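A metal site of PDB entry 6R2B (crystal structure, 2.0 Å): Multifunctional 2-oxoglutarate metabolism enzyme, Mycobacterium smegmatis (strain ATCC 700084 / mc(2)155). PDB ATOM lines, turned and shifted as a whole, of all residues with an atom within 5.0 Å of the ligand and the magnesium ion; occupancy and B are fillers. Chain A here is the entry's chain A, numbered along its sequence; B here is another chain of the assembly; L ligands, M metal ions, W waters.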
ATOM      1  N   LYS A 145      -1.331   3.121   3.596  1.00  0.00           N
ATOM      2  CA  LYS A 145      -2.073   3.051   4.866  1.00  0.00           C
ATOM      3  C   LYS A 145      -3.056   1.907   4.896  1.00  0.00           C
ATOM      4  O   LYS A 145      -3.961   1.839   4.057  1.00  0.00           O
ATOM      5  CB  LYS A 145      -2.816   4.358   5.146  1.00  0.00           C
ATOM      6  CG  LYS A 145      -2.125   5.268   6.148  1.00  0.00           C
ATOM      7  CD  LYS A 145      -2.989   6.467   6.505  1.00  0.00           C
ATOM      8  CE  LYS A 145      -2.113   7.641   6.803  1.00  0.00           C
ATOM      9  NZ  LYS A 145      -2.848   8.711   7.540  1.00  0.00           N
ATOM     10  N   PHE A 147      -3.363   0.367   8.510  1.00  0.00           N
ATOM     11  CA  PHE A 147      -3.450   0.246   9.977  1.00  0.00           C
ATOM     12  C   PHE A 147      -3.549  -1.215  10.383  1.00  0.00           C
ATOM     13  O   PHE A 147      -4.540  -1.659  10.994  1.00  0.00           O
ATOM     14  CB  PHE A 147      -4.606   1.058  10.582  1.00  0.00           C
ATOM     15  CG  PHE A 147      -4.407   2.541  10.477  1.00  0.00           C
ATOM     16  CD1 PHE A 147      -3.449   3.196  11.246  1.00  0.00           C
ATOM     17  CD2 PHE A 147      -5.208   3.308   9.615  1.00  0.00           C
ATOM     18  CE1 PHE A 147      -3.268   4.574  11.146  1.00  0.00           C
ATOM     19  CE2 PHE A 147      -5.005   4.695   9.500  1.00  0.00           C
ATOM     20  CZ  PHE A 147      -4.056   5.323  10.279  1.00  0.00           C
ATOM     21  N   HIS A 180      -9.917   1.983  13.419  1.00  0.00           N
ATOM     22  CA  HIS A 180      -9.014   1.636  12.311  1.00  0.00           C
ATOM     23  C   HIS A 180      -8.135   0.386  12.516  1.00  0.00           C
ATOM     24  O   HIS A 180      -7.822  -0.261  11.536  1.00  0.00           O
ATOM     25  CB  HIS A 180      -8.080   2.826  12.056  1.00  0.00           C
ATOM     26  CG  HIS A 180      -7.353   3.278  13.288  1.00  0.00           C
ATOM     27  ND1 HIS A 180      -8.011   3.935  14.317  1.00  0.00           N
ATOM     28  CD2 HIS A 180      -6.054   3.111  13.652  1.00  0.00           C
ATOM     29  CE1 HIS A 180      -7.105   4.172  15.245  1.00  0.00           C
ATOM     30  NE2 HIS A 180      -5.917   3.697  14.905  1.00  0.00           N
ATOM     31  N   ARG A 181      -7.683   0.092  13.752  1.00  0.00           N
ATOM     32  CA  ARG A 181      -6.739  -1.010  14.023  1.00  0.00           C
ATOM     33  C   ARG A 181      -7.298  -2.381  13.630  1.00  0.00           C
ATOM     34  O   ARG A 181      -8.159  -2.909  14.296  1.00  0.00           O
ATOM     35  CB  ARG A 181      -6.323  -0.997  15.523  1.00  0.00           C
ATOM     36  CG  ARG A 181      -5.032  -1.783  15.889  1.00  0.00           C
ATOM     37  CD  ARG A 181      -3.811  -1.419  15.050  1.00  0.00           C
ATOM     38  NE  ARG A 181      -3.434  -0.004  15.180  1.00  0.00           N
ATOM     39  CZ  ARG A 181      -2.530   0.612  14.428  1.00  0.00           C
ATOM     40  NH1 ARG A 181      -1.907  -0.045  13.454  1.00  0.00           N
ATOM     41  NH2 ARG A 181      -2.233   1.889  14.651  1.00  0.00           N
ATOM     42  N   TYR A 219     -10.731   2.094   5.637  1.00  0.00           N
ATOM     43  CA  TYR A 219     -10.760   1.637   7.020  1.00  0.00           C
ATOM     44  C   TYR A 219     -11.934   2.277   7.806  1.00  0.00           C
ATOM     45  O   TYR A 219     -11.993   2.177   9.029  1.00  0.00           O
ATOM     46  CB  TYR A 219      -9.401   1.852   7.731  1.00  0.00           C
ATOM     47  CG  TYR A 219      -8.716   3.164   7.439  1.00  0.00           C
ATOM     48  CD1 TYR A 219      -9.037   4.316   8.164  1.00  0.00           C
ATOM     49  CD2 TYR A 219      -7.691   3.252   6.491  1.00  0.00           C
ATOM     50  CE1 TYR A 219      -8.367   5.514   7.946  1.00  0.00           C
ATOM     51  CE2 TYR A 219      -7.041   4.460   6.248  1.00  0.00           C
ATOM     52  CZ  TYR A 219      -7.394   5.586   6.962  1.00  0.00           C
ATOM     53  OH  TYR A 219      -6.764   6.779   6.721  1.00  0.00           O
ATOM     54  N   HIS A 220     -12.925   2.841   7.089  1.00  0.00           N
ATOM     55  CA  HIS A 220     -14.139   3.399   7.712  1.00  0.00           C
ATOM     56  C   HIS A 220     -15.381   2.704   7.246  1.00  0.00           C
ATOM     57  O   HIS A 220     -16.473   3.043   7.681  1.00  0.00           O
ATOM     58  CB  HIS A 220     -14.282   4.891   7.362  1.00  0.00           C
ATOM     59  CG  HIS A 220     -13.347   5.786   8.116  1.00  0.00           C
ATOM     60  ND1 HIS A 220     -13.339   7.137   7.899  1.00  0.00           N
ATOM     61  CD2 HIS A 220     -12.401   5.467   9.018  1.00  0.00           C
ATOM     62  CE1 HIS A 220     -12.378   7.612   8.673  1.00  0.00           C
ATOM     63  NE2 HIS A 220     -11.769   6.642   9.354  1.00  0.00           N
ATOM     64  N   PRO A 244     -16.637   7.672  11.232  1.00  0.00           N
ATOM     65  CA  PRO A 244     -15.661   8.660  10.786  1.00  0.00           C
ATOM     66  C   PRO A 244     -14.312   8.376  11.457  1.00  0.00           C
ATOM     67  O   PRO A 244     -14.202   7.424  12.241  1.00  0.00           O
ATOM     68  CB  PRO A 244     -16.275   9.981  11.258  1.00  0.00           C
ATOM     69  CG  PRO A 244     -17.003   9.608  12.546  1.00  0.00           C
ATOM     70  CD  PRO A 244     -17.403   8.154  12.413  1.00  0.00           C
ATOM     71  N   SER A 245     -13.315   9.235  11.196  1.00  0.00           N
ATOM     72  CA  SER A 245     -11.997   9.116  11.822  1.00  0.00           C
ATOM     73  C   SER A 245     -12.108   9.367  13.324  1.00  0.00           C
ATOM     74  O   SER A 245     -11.373   8.754  14.083  1.00  0.00           O
ATOM     75  CB  SER A 245     -11.013  10.085  11.187  1.00  0.00           C
ATOM     76  OG  SER A 245     -10.530   9.693   9.912  1.00  0.00           O
ATOM     77  N   HIS A 246     -13.050  10.236  13.747  1.00  0.00           N
ATOM     78  CA  HIS A 246     -13.298  10.630  15.164  1.00  0.00           C
ATOM     79  C   HIS A 246     -13.480   9.397  16.027  1.00  0.00           C
ATOM     80  O   HIS A 246     -14.507   8.707  15.961  1.00  0.00           O
ATOM     81  CB  HIS A 246     -14.501  11.578  15.248  1.00  0.00           C
ATOM     82  CG  HIS A 246     -14.261  12.878  14.527  1.00  0.00           C
ATOM     83  ND1 HIS A 246     -13.946  12.903  13.176  1.00  0.00           N
ATOM     84  CD2 HIS A 246     -14.284  14.141  15.000  1.00  0.00           C
ATOM     85  CE1 HIS A 246     -13.780  14.187  12.877  1.00  0.00           C
ATOM     86  NE2 HIS A 246     -13.980  14.969  13.933  1.00  0.00           N
ATOM     87  N   LEU A 247     -12.415   9.054  16.745  1.00  0.00           N
ATOM     88  CA  LEU A 247     -12.344   7.846  17.561  1.00  0.00           C
ATOM     89  C   LEU A 247     -13.369   7.916  18.658  1.00  0.00           C
ATOM     90  O   LEU A 247     -13.535   8.963  19.285  1.00  0.00           O
ATOM     91  CB  LEU A 247     -10.929   7.622  18.124  1.00  0.00           C
ATOM     92  CG  LEU A 247      -9.767   7.554  17.075  1.00  0.00           C
ATOM     93  CD1 LEU A 247      -8.403   7.645  17.733  1.00  0.00           C
ATOM     94  CD2 LEU A 247      -9.836   6.326  16.252  1.00  0.00           C
ATOM     95  N   GLY A 285      -9.348   1.463  20.815  1.00  0.00           N
ATOM     96  CA  GLY A 285      -7.899   1.564  20.929  1.00  0.00           C
ATOM     97  C   GLY A 285      -7.641   2.035  22.352  1.00  0.00           C
ATOM     98  O   GLY A 285      -8.521   2.662  22.943  1.00  0.00           O
ATOM     99  N   ASP A 286      -6.459   1.741  22.924  1.00  0.00           N
ATOM    100  CA  ASP A 286      -6.136   2.087  24.318  1.00  0.00           C
ATOM    101  C   ASP A 286      -6.095   3.607  24.605  1.00  0.00           C
ATOM    102  O   ASP A 286      -6.576   4.003  25.655  1.00  0.00           O
ATOM    103  CB  ASP A 286      -4.817   1.410  24.790  1.00  0.00           C
ATOM    104  CG  ASP A 286      -3.570   1.673  23.918  1.00  0.00           C
ATOM    105  OD1 ASP A 286      -3.627   1.384  22.721  1.00  0.00           O
ATOM    106  OD2 ASP A 286      -2.529   2.104  24.475  1.00  0.00           O
ATOM    107  N   ALA A 287      -5.445   4.421  23.747  1.00  0.00           N
ATOM    108  CA  ALA A 287      -5.350   5.871  24.049  1.00  0.00           C
ATOM    109  C   ALA A 287      -6.713   6.539  23.897  1.00  0.00           C
ATOM    110  O   ALA A 287      -7.067   7.343  24.746  1.00  0.00           O
ATOM    111  CB  ALA A 287      -4.314   6.555  23.160  1.00  0.00           C
ATOM    112  N   ALA A 288      -7.510   6.134  22.874  1.00  0.00           N
ATOM    113  CA  ALA A 288      -8.831   6.715  22.654  1.00  0.00           C
ATOM    114  C   ALA A 288      -9.834   6.341  23.764  1.00  0.00           C
ATOM    115  O   ALA A 288     -10.630   7.203  24.161  1.00  0.00           O
ATOM    116  CB  ALA A 288      -9.372   6.283  21.297  1.00  0.00           C
ATOM    117  N   GLN A 292     -11.264   9.907  25.330  1.00  0.00           N
ATOM    118  CA  GLN A 292     -12.505  10.459  24.727  1.00  0.00           C
ATOM    119  C   GLN A 292     -13.726  10.367  25.685  1.00  0.00           C
ATOM    120  O   GLN A 292     -14.131   9.286  26.080  1.00  0.00           O
ATOM    121  CB  GLN A 292     -12.810   9.756  23.394  1.00  0.00           C
ATOM    122  CG  GLN A 292     -11.815  10.135  22.287  1.00  0.00           C
ATOM    123  CD  GLN A 292     -12.053  11.548  21.759  1.00  0.00           C
ATOM    124  OE1 GLN A 292     -13.151  11.925  21.336  1.00  0.00           O
ATOM    125  NE2 GLN A 292     -11.017  12.363  21.776  1.00  0.00           N
ATOM    126  N   VAL A 317      -8.139  -3.068  21.990  1.00  0.00           N
ATOM    127  CA  VAL A 317      -6.910  -3.560  21.348  1.00  0.00           C
ATOM    128  C   VAL A 317      -5.804  -2.726  21.988  1.00  0.00           C
ATOM    129  O   VAL A 317      -5.462  -1.641  21.512  1.00  0.00           O
ATOM    130  CB  VAL A 317      -6.945  -3.440  19.789  1.00  0.00           C
ATOM    131  CG1 VAL A 317      -5.685  -4.027  19.166  1.00  0.00           C
ATOM    132  CG2 VAL A 317      -8.196  -4.088  19.203  1.00  0.00           C
ATOM    133  N   ASN A 319      -2.475  -2.054  22.435  1.00  0.00           N
ATOM    134  CA  ASN A 319      -1.108  -2.230  21.893  1.00  0.00           C
ATOM    135  C   ASN A 319      -0.103  -1.301  22.624  1.00  0.00           C
ATOM    136  O   ASN A 319       1.016  -1.127  22.170  1.00  0.00           O
ATOM    137  CB  ASN A 319      -1.084  -1.993  20.374  1.00  0.00           C
ATOM    138  CG  ASN A 319      -1.842  -0.780  19.951  1.00  0.00           C
ATOM    139  OD1 ASN A 319      -2.016   0.161  20.707  1.00  0.00           O
ATOM    140  ND2 ASN A 319      -2.352  -0.794  18.741  1.00  0.00           N
ATOM    141  N   GLN A 320      -0.520  -0.759  23.765  1.00  0.00           N
ATOM    142  CA  GLN A 320       0.287   0.005  24.734  1.00  0.00           C
ATOM    143  C   GLN A 320       1.012   1.220  24.105  1.00  0.00           C
ATOM    144  O   GLN A 320       2.112   1.580  24.535  1.00  0.00           O
ATOM    145  CB  GLN A 320       1.285  -0.954  25.430  1.00  0.00           C
ATOM    146  CG  GLN A 320       0.612  -2.229  25.979  1.00  0.00           C
ATOM    147  CD  GLN A 320       1.613  -3.219  26.539  1.00  0.00           C
ATOM    148  OE1 GLN A 320       2.263  -2.972  27.545  1.00  0.00           O
ATOM    149  NE2 GLN A 320       1.774  -4.349  25.868  1.00  0.00           N
ATOM    150  N   ILE A 321       0.363   1.858  23.139  1.00  0.00           N
ATOM    151  CA  ILE A 321       0.818   3.055  22.415  1.00  0.00           C
ATOM    152  C   ILE A 321      -0.365   3.693  21.705  1.00  0.00           C
ATOM    153  O   ILE A 321      -1.297   2.994  21.291  1.00  0.00           O
ATOM    154  CB  ILE A 321       1.969   2.666  21.402  1.00  0.00           C
ATOM    155  CG1 ILE A 321       2.667   3.884  20.789  1.00  0.00           C
ATOM    156  CG2 ILE A 321       1.494   1.689  20.284  1.00  0.00           C
ATOM    157  CD1 ILE A 321       3.632   4.495  21.596  1.00  0.00           C
ATOM    158  N   GLY A 322      -0.281   5.025  21.540  1.00  0.00           N
ATOM    159  CA  GLY A 322      -1.224   5.826  20.779  1.00  0.00           C
ATOM    160  C   GLY A 322      -0.389   6.659  19.821  1.00  0.00           C
ATOM    161  O   GLY A 322       0.099   7.712  20.203  1.00  0.00           O
ATOM    162  N   PHE A 323      -0.141   6.158  18.597  1.00  0.00           N
ATOM    163  CA  PHE A 323       0.697   6.836  17.592  1.00  0.00           C
ATOM    164  C   PHE A 323       2.131   6.929  18.115  1.00  0.00           C
ATOM    165  O   PHE A 323       2.815   5.903  18.128  1.00  0.00           O
ATOM    166  CB  PHE A 323       0.119   8.226  17.210  1.00  0.00           C
ATOM    167  CG  PHE A 323       0.558   8.813  15.880  1.00  0.00           C
ATOM    168  CD1 PHE A 323       1.746   8.396  15.273  1.00  0.00           C
ATOM    169  CD2 PHE A 323      -0.203   9.788  15.241  1.00  0.00           C
ATOM    170  CE1 PHE A 323       2.126   8.905  14.038  1.00  0.00           C
ATOM    171  CE2 PHE A 323       0.193  10.303  14.008  1.00  0.00           C
ATOM    172  CZ  PHE A 323       1.360   9.869  13.427  1.00  0.00           C
ATOM    173  N   HIS A 388       2.684   3.440  13.594  1.00  0.00           N
ATOM    174  CA  HIS A 388       1.261   3.779  13.767  1.00  0.00           C
ATOM    175  C   HIS A 388       0.477   3.458  12.500  1.00  0.00           C
ATOM    176  O   HIS A 388      -0.608   2.855  12.548  1.00  0.00           O
ATOM    177  CB  HIS A 388       1.118   5.254  14.088  1.00  0.00           C
ATOM    178  CG  HIS A 388      -0.296   5.680  14.230  1.00  0.00           C
ATOM    179  ND1 HIS A 388      -1.151   5.053  15.118  1.00  0.00           N
ATOM    180  CD2 HIS A 388      -0.956   6.688  13.631  1.00  0.00           C
ATOM    181  CE1 HIS A 388      -2.295   5.686  14.996  1.00  0.00           C
ATOM    182  NE2 HIS A 388      -2.206   6.697  14.143  1.00  0.00           N
ATOM    183  N   GLN B 542      -1.763  16.370  20.172  1.00  0.00           N
ATOM    184  CA  GLN B 542      -1.568  14.950  19.870  1.00  0.00           C
ATOM    185  C   GLN B 542      -0.314  14.717  19.040  1.00  0.00           C
ATOM    186  O   GLN B 542      -0.206  15.214  17.897  1.00  0.00           O
ATOM    187  CB  GLN B 542      -2.817  14.367  19.190  1.00  0.00           C
ATOM    188  CG  GLN B 542      -3.923  14.043  20.212  1.00  0.00           C
ATOM    189  CD  GLN B 542      -5.309  14.121  19.621  1.00  0.00           C
ATOM    190  OE1 GLN B 542      -5.526  13.865  18.443  1.00  0.00           O
ATOM    191  NE2 GLN B 542      -6.295  14.466  20.438  1.00  0.00           N
ATOM    192  N   ASP B 543       0.665  14.032  19.667  1.00  0.00           N
ATOM    193  CA  ASP B 543       1.992  13.676  19.119  1.00  0.00           C
ATOM    194  C   ASP B 543       2.781  14.941  18.715  1.00  0.00           C
ATOM    195  O   ASP B 543       3.572  14.907  17.785  1.00  0.00           O
ATOM    196  CB  ASP B 543       1.790  12.703  17.946  1.00  0.00           C
ATOM    197  CG  ASP B 543       0.939  11.519  18.386  1.00  0.00           C
ATOM    198  OD1 ASP B 543       1.441  10.679  19.155  1.00  0.00           O
ATOM    199  OD2 ASP B 543      -0.256  11.469  17.996  1.00  0.00           O
ATOM    200  N   LEU B 591      -5.442  11.780  24.355  1.00  0.00           N
ATOM    201  CA  LEU B 591      -6.235  11.785  23.133  1.00  0.00           C
ATOM    202  C   LEU B 591      -7.600  12.401  23.437  1.00  0.00           C
ATOM    203  O   LEU B 591      -8.626  11.712  23.523  1.00  0.00           O
ATOM    204  CB  LEU B 591      -6.374  10.378  22.545  1.00  0.00           C
ATOM    205  CG  LEU B 591      -6.356  10.274  21.016  1.00  0.00           C
ATOM    206  CD1 LEU B 591      -6.088   8.863  20.599  1.00  0.00           C
ATOM    207  CD2 LEU B 591      -7.662  10.759  20.380  1.00  0.00           C
ATOM    208  N   GLU B 593      -9.827  16.381  22.836  1.00  0.00           N
ATOM    209  CA  GLU B 593      -9.932  17.676  22.156  1.00  0.00           C
ATOM    210  C   GLU B 593     -10.643  18.618  23.111  1.00  0.00           C
ATOM    211  O   GLU B 593     -10.070  19.640  23.495  1.00  0.00           O
ATOM    212  CB  GLU B 593     -10.641  17.582  20.784  1.00  0.00           C
ATOM    213  CG  GLU B 593      -9.791  17.008  19.650  1.00  0.00           C
ATOM    214  CD  GLU B 593      -9.708  15.490  19.607  1.00  0.00           C
ATOM    215  OE1 GLU B 593      -8.752  14.967  18.977  1.00  0.00           O
ATOM    216  OE2 GLU B 593     -10.577  14.827  20.206  1.00  0.00           O
ATOM    217  N   GLN B 617      -4.332  17.230  15.751  1.00  0.00           N
ATOM    218  CA  GLN B 617      -3.586  16.264  14.944  1.00  0.00           C
ATOM    219  C   GLN B 617      -3.825  16.646  13.461  1.00  0.00           C
ATOM    220  O   GLN B 617      -2.884  16.788  12.660  1.00  0.00           O
ATOM    221  CB  GLN B 617      -4.018  14.824  15.261  1.00  0.00           C
ATOM    222  CG  GLN B 617      -3.218  13.834  14.414  1.00  0.00           C
ATOM    223  CD  GLN B 617      -2.590  12.736  15.222  1.00  0.00           C
ATOM    224  OE1 GLN B 617      -2.980  11.594  15.114  1.00  0.00           O
ATOM    225  NE2 GLN B 617      -1.583  13.047  15.996  1.00  0.00           N
ATOM    226  N   PHE B 618      -5.107  16.861  13.150  1.00  0.00           N
ATOM    227  CA  PHE B 618      -5.668  17.379  11.894  1.00  0.00           C
ATOM    228  C   PHE B 618      -6.767  18.327  12.314  1.00  0.00           C
ATOM    229  O   PHE B 618      -7.492  18.000  13.253  1.00  0.00           O
ATOM    230  CB  PHE B 618      -6.201  16.245  10.989  1.00  0.00           C
ATOM    231  CG  PHE B 618      -5.128  15.396  10.356  1.00  0.00           C
ATOM    232  CD1 PHE B 618      -4.561  14.319  11.045  1.00  0.00           C
ATOM    233  CD2 PHE B 618      -4.668  15.673   9.066  1.00  0.00           C
ATOM    234  CE1 PHE B 618      -3.539  13.547  10.476  1.00  0.00           C
ATOM    235  CE2 PHE B 618      -3.675  14.883   8.482  1.00  0.00           C
ATOM    236  CZ  PHE B 618      -3.111  13.828   9.192  1.00  0.00           C
ATOM    237  N   PHE B 621     -10.472  17.423  13.651  1.00  0.00           N
ATOM    238  CA  PHE B 621     -10.862  16.891  14.966  1.00  0.00           C
ATOM    239  C   PHE B 621     -11.191  17.989  15.987  1.00  0.00           C
ATOM    240  O   PHE B 621     -11.716  17.661  17.054  1.00  0.00           O
ATOM    241  CB  PHE B 621      -9.768  15.951  15.509  1.00  0.00           C
ATOM    242  CG  PHE B 621      -9.500  14.796  14.580  1.00  0.00           C
ATOM    243  CD1 PHE B 621     -10.498  13.864  14.292  1.00  0.00           C
ATOM    244  CD2 PHE B 621      -8.266  14.667  13.944  1.00  0.00           C
ATOM    245  CE1 PHE B 621     -10.278  12.843  13.369  1.00  0.00           C
ATOM    246  CE2 PHE B 621      -8.035  13.634  13.030  1.00  0.00           C
ATOM    247  CZ  PHE B 621      -9.038  12.730  12.751  1.00  0.00           C
ATOM    248  N   HIS B 661      -9.403  14.312   7.088  1.00  0.00           N
ATOM    249  CA  HIS B 661      -7.995  14.687   6.992  1.00  0.00           C
ATOM    250  C   HIS B 661      -7.867  15.766   5.941  1.00  0.00           C
ATOM    251  O   HIS B 661      -6.924  15.743   5.154  1.00  0.00           O
ATOM    252  CB  HIS B 661      -7.117  13.484   6.639  1.00  0.00           C
ATOM    253  CG  HIS B 661      -7.054  12.449   7.723  1.00  0.00           C
ATOM    254  ND1 HIS B 661      -8.036  11.489   7.851  1.00  0.00           N
ATOM    255  CD2 HIS B 661      -6.132  12.269   8.699  1.00  0.00           C
ATOM    256  CE1 HIS B 661      -7.681  10.748   8.890  1.00  0.00           C
ATOM    257  NE2 HIS B 661      -6.562  11.200   9.457  1.00  0.00           N
HETATM  258  N1  LIG L   1      -8.924  12.748  17.652  1.00  0.00           N
HETATM  259  C1  LIG L   1      -9.995  11.972  17.345  1.00  0.00           C
HETATM  260  C2  LIG L   1     -11.279  12.249  18.115  1.00  0.00           C
HETATM  261  N2  LIG L   1     -10.064  10.951  16.441  1.00  0.00           N
HETATM  262  C3  LIG L   1      -8.885  10.729  15.748  1.00  0.00           C
HETATM  263  N3  LIG L   1      -8.990   9.799  14.721  1.00  0.00           N
HETATM  264  C4  LIG L   1      -7.667  11.486  15.995  1.00  0.00           C
HETATM  265  C5  LIG L   1      -7.751  12.495  16.956  1.00  0.00           C
HETATM  266  C6  LIG L   1      -6.395  11.256  15.248  1.00  0.00           C
HETATM  267  N4  LIG L   1      -5.800   9.904  15.449  1.00  0.00           N
HETATM  268  C7  LIG L   1      -6.153   8.828  14.487  1.00  0.00           C
HETATM  269  S1  LIG L   1      -5.436   7.241  15.195  1.00  0.00           S
HETATM  270  C8  LIG L   1      -4.775   8.149  16.637  1.00  0.00           C
HETATM  271  C9  LIG L   1      -5.079   9.507  16.614  1.00  0.00           C
HETATM  272  C10 LIG L   1      -4.677  10.527  17.686  1.00  0.00           C
HETATM  273  C11 LIG L   1      -4.061   7.431  17.695  1.00  0.00           C
HETATM  274  C12 LIG L   1      -4.953   6.293  18.304  1.00  0.00           C
HETATM  275  O1  LIG L   1      -4.352   5.628  19.302  1.00  0.00           O
HETATM  276  P1  LIG L   1      -5.082   4.230  19.976  1.00  0.00           P
HETATM  277  O2  LIG L   1      -4.120   3.743  21.049  1.00  0.00           O
HETATM  278  O3  LIG L   1      -6.411   4.689  20.378  1.00  0.00           O
HETATM  279  O4  LIG L   1      -5.254   3.361  18.720  1.00  0.00           O
HETATM  280  P2  LIG L   1      -4.087   2.481  17.862  1.00  0.00           P
HETATM  281  O5  LIG L   1      -3.746   3.306  16.645  1.00  0.00           O
HETATM  282  O6  LIG L   1      -2.900   2.376  18.786  1.00  0.00           O
HETATM  283  O7  LIG L   1      -4.760   1.174  17.467  1.00  0.00           O
HETATM  284  C13 LIG L   1      -5.989   9.003  12.966  1.00  0.00           C
HETATM  285  P3  LIG L   1      -4.348   9.755  12.214  1.00  0.00           P
HETATM  286  O8  LIG L   1      -4.620   9.785  10.728  1.00  0.00           O
HETATM  287  O9  LIG L   1      -4.247  11.089  12.931  1.00  0.00           O
HETATM  288  O10 LIG L   1      -3.265   8.785  12.639  1.00  0.00           O
HETATM  289  C14 LIG L   1      -6.128   7.562  12.290  1.00  0.00           C
HETATM  290  O11 LIG L   1      -7.062   9.810  12.539  1.00  0.00           O
HETATM  291  C15 LIG L   1      -7.457   6.811  12.365  1.00  0.00           C
HETATM  292  C16 LIG L   1      -8.539   7.287  11.388  1.00  0.00           C
HETATM  293  O12 LIG L   1      -8.392   8.375  10.793  1.00  0.00           O
HETATM  294  O13 LIG L   1      -9.542   6.561  11.162  1.00  0.00           O
HETATM  295 MG    MG M   1      -3.007   1.876  20.960  1.00  0.00          MG
HETATM  296  O   HOH W   1     -12.675  15.285  18.060  1.00  0.00           O
HETATM  297  O   HOH W   2      -5.448   8.398   8.432  1.00  0.00           O
HETATM  298  O   HOH W   3      -4.799   0.738  20.259  1.00  0.00           O
HETATM  299  O   HOH W   4     -10.479   5.046  13.079  1.00  0.00           O
HETATM  300  O   HOH W   5      -7.646   1.533  17.385  1.00  0.00           O
HETATM  301  O   HOH W   6      -1.862   9.918  19.563  1.00  0.00           O
HETATM  302  O   HOH W   7      -1.908   8.015  10.384  1.00  0.00           O
HETATM  303  O   HOH W   8      -0.942   3.643  17.492  1.00  0.00           O
HETATM  304  O   HOH W   9      -8.367   3.999  18.621  1.00  0.00           O
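The side-chain amide oxygen of Gln 617 of chain B sits close to an oxygen (O9) of the ligand, at 2.6 Å. OE1 of Glu 593 of chain B sits at hydrogen-bond distance from N1 of the ligand (2.6 Å). O of Ser 245 sits at hydrogen-bond distance from N3 of the ligand (2.7 Å). The side-chain hydroxyl (OG) of Ser 245 lies within hydrogen-bond range of an oxygen (O12) of the ligand (2.7 Å). An oxygen (O8) of the ligand is in hydrogen-bond range of a ring nitrogen (NE2) of His 661 of chain B. A ring nitrogen (NE2) of His 388 is in hydrogen-bond range of an oxygen (O10) of the ligand. O5 of the ligand sits at hydrogen-bond distance from NE2 of His 180 (2.8 Å). NE2 of His 220 lies within hydrogen-bond range of O13 of the ligand (2.9 Å). An oxygen (O5) of the ligand is in salt-bridge range of the guanidinium group (NH2) of Arg 181 (2.9 Å). The backbone NH of Leu 247 is in hydrogen-bond range of a nitrogen (N2) of the ligand (3.0 Å). O2 of the ligand sits close to N of Ala 287, at 3.1 Å. An oxygen (O3) of the ligand lies within hydrogen-bond range of the backbone NH (N) of Ala 288 (3.1 Å). The side-chain amino group (NZ) of Lys 145 lies within salt-bridge range of an oxygen (O8) of the ligand (3.8 Å).
The side-chain amide nitrogen (NE2) of Gln 617 of chain B is in hydrogen-bond range of the backbone carbonyl oxygen (O) of Gln 542 of chain B (3.2 Å). The side-chain carboxylate of Asp 543 of chain B sits at hydrogen-bond distance from the side-chain amide nitrogen of Gln 617 of chain B, at 2.9 Å. The side-chain carboxylate of Glu 593 of chain B lies within hydrogen-bond range of the side-chain amide nitrogen of Gln 542 of chain B. The side-chain carboxylate (OE2) of Glu 593 of chain B is in hydrogen-bond range of the side-chain amide nitrogen (NE2) of Gln 292. OG of Ser 245 sits close to NE2 of His 220 (3.3 Å). The guanidinium group of Arg 181 sits at hydrogen-bond distance from the backbone carbonyl oxygen of His 388 (2.8 Å). O of Leu 591 of chain B is in hydrogen-bond range of NE2 of Gln 292 (3.0 Å).
Phe 147 touches the ligand (CZ to C14, 3.7 Å). Tyr 219 touches the ligand (CE1 to O13, 3.6 Å). His 246 touches the ligand (CA to N2, 3.5 Å). Gly 285 touches the ligand. NE2 of Gln 292 touches C2 of the ligand (3.7 Å). Gly 322 touches the ligand. Gln 542 of chain B touches the ligand. Leu 591 of chain B touches the ligand. CE1 of Phe 618 of chain B touches O9 of the ligand, at 3.5 Å. CE1 of Phe 621 of chain B touches C3 of the ligand (3.5 Å). Hydrophobic or aromatic side chains that line the ligand: Phe 147, His 180, Tyr 219, His 220, Leu 247, Ala 287, Ala 288, His 388, Leu 591 of chain B, Phe 618 of chain B, Phe 621 of chain B and His 661 of chain B. Within 4 Å of the ligand: Lys 145, Phe 147, His 180, Arg 181, Tyr 219, His 220, Ser 245, His 246, Leu 247, Gly 285, Asp 286, Ala 287, Ala 288, Gln 292, Asn 319, Ile 321, Gly 322, His 388, Gln 542 of chain B, Leu 591 of chain B, Glu 593 of chain B, Gln 617 of chain B, Phe 618 of chain B, Phe 621 of chain B and His 661 of chain B. The nearest printed residue that does not touch the ligand is Phe 323 (4.02 Å).
Three residues have an atom within 4 Å of the magnesium ion: Asp 286, Asn 319 and Ile 321.
The magnesium ion is bound by the side-chain carboxylate (OD1) of Asp 286 (1.9 Å), the side-chain amide oxygen (OD1) of Asn 319 (2.0 Å), the backbone carbonyl oxygen (O) of Ile 321 (2.1 Å), an oxygen (O2) of the ligand (2.2 Å), an oxygen (O6) of the ligand (2.2 Å) and water W3 (2.2 Å). The magnesium ion has six donor atoms within binding distance.
Water W3 lies within hydrogen-bond range of O of Val 317 (2.8 Å), O7 of the ligand (2.8 Å), ND2 of Asn 319 (3.3 Å) and N of Asp 286 (3.3 Å). Water W4 bridges O13 of the ligand (2.6 Å) and ND1 of His 180 (3.0 Å). Water W8 lies within hydrogen-bond range of ND1 of His 388, N of Phe 323 and O5 of the ligand. Water W9 bridges an oxygen (O3) of the ligand (2.7 Å) and the backbone NH (N) of Gly 285 (3.5 Å). Water W2 lies within hydrogen-bond range of OH of Tyr 219 (2.7 Å), NZ of Lys 145 (2.8 Å), O8 of the ligand (2.8 Å) and NE2 of His 661 of chain B (3.2 Å). Water W1 bridges the backbone carbonyl oxygen (O) of Phe 621 of chain B (2.8 Å) and the side-chain carboxylate (OE2) of Glu 593 of chain B (3.0 Å).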
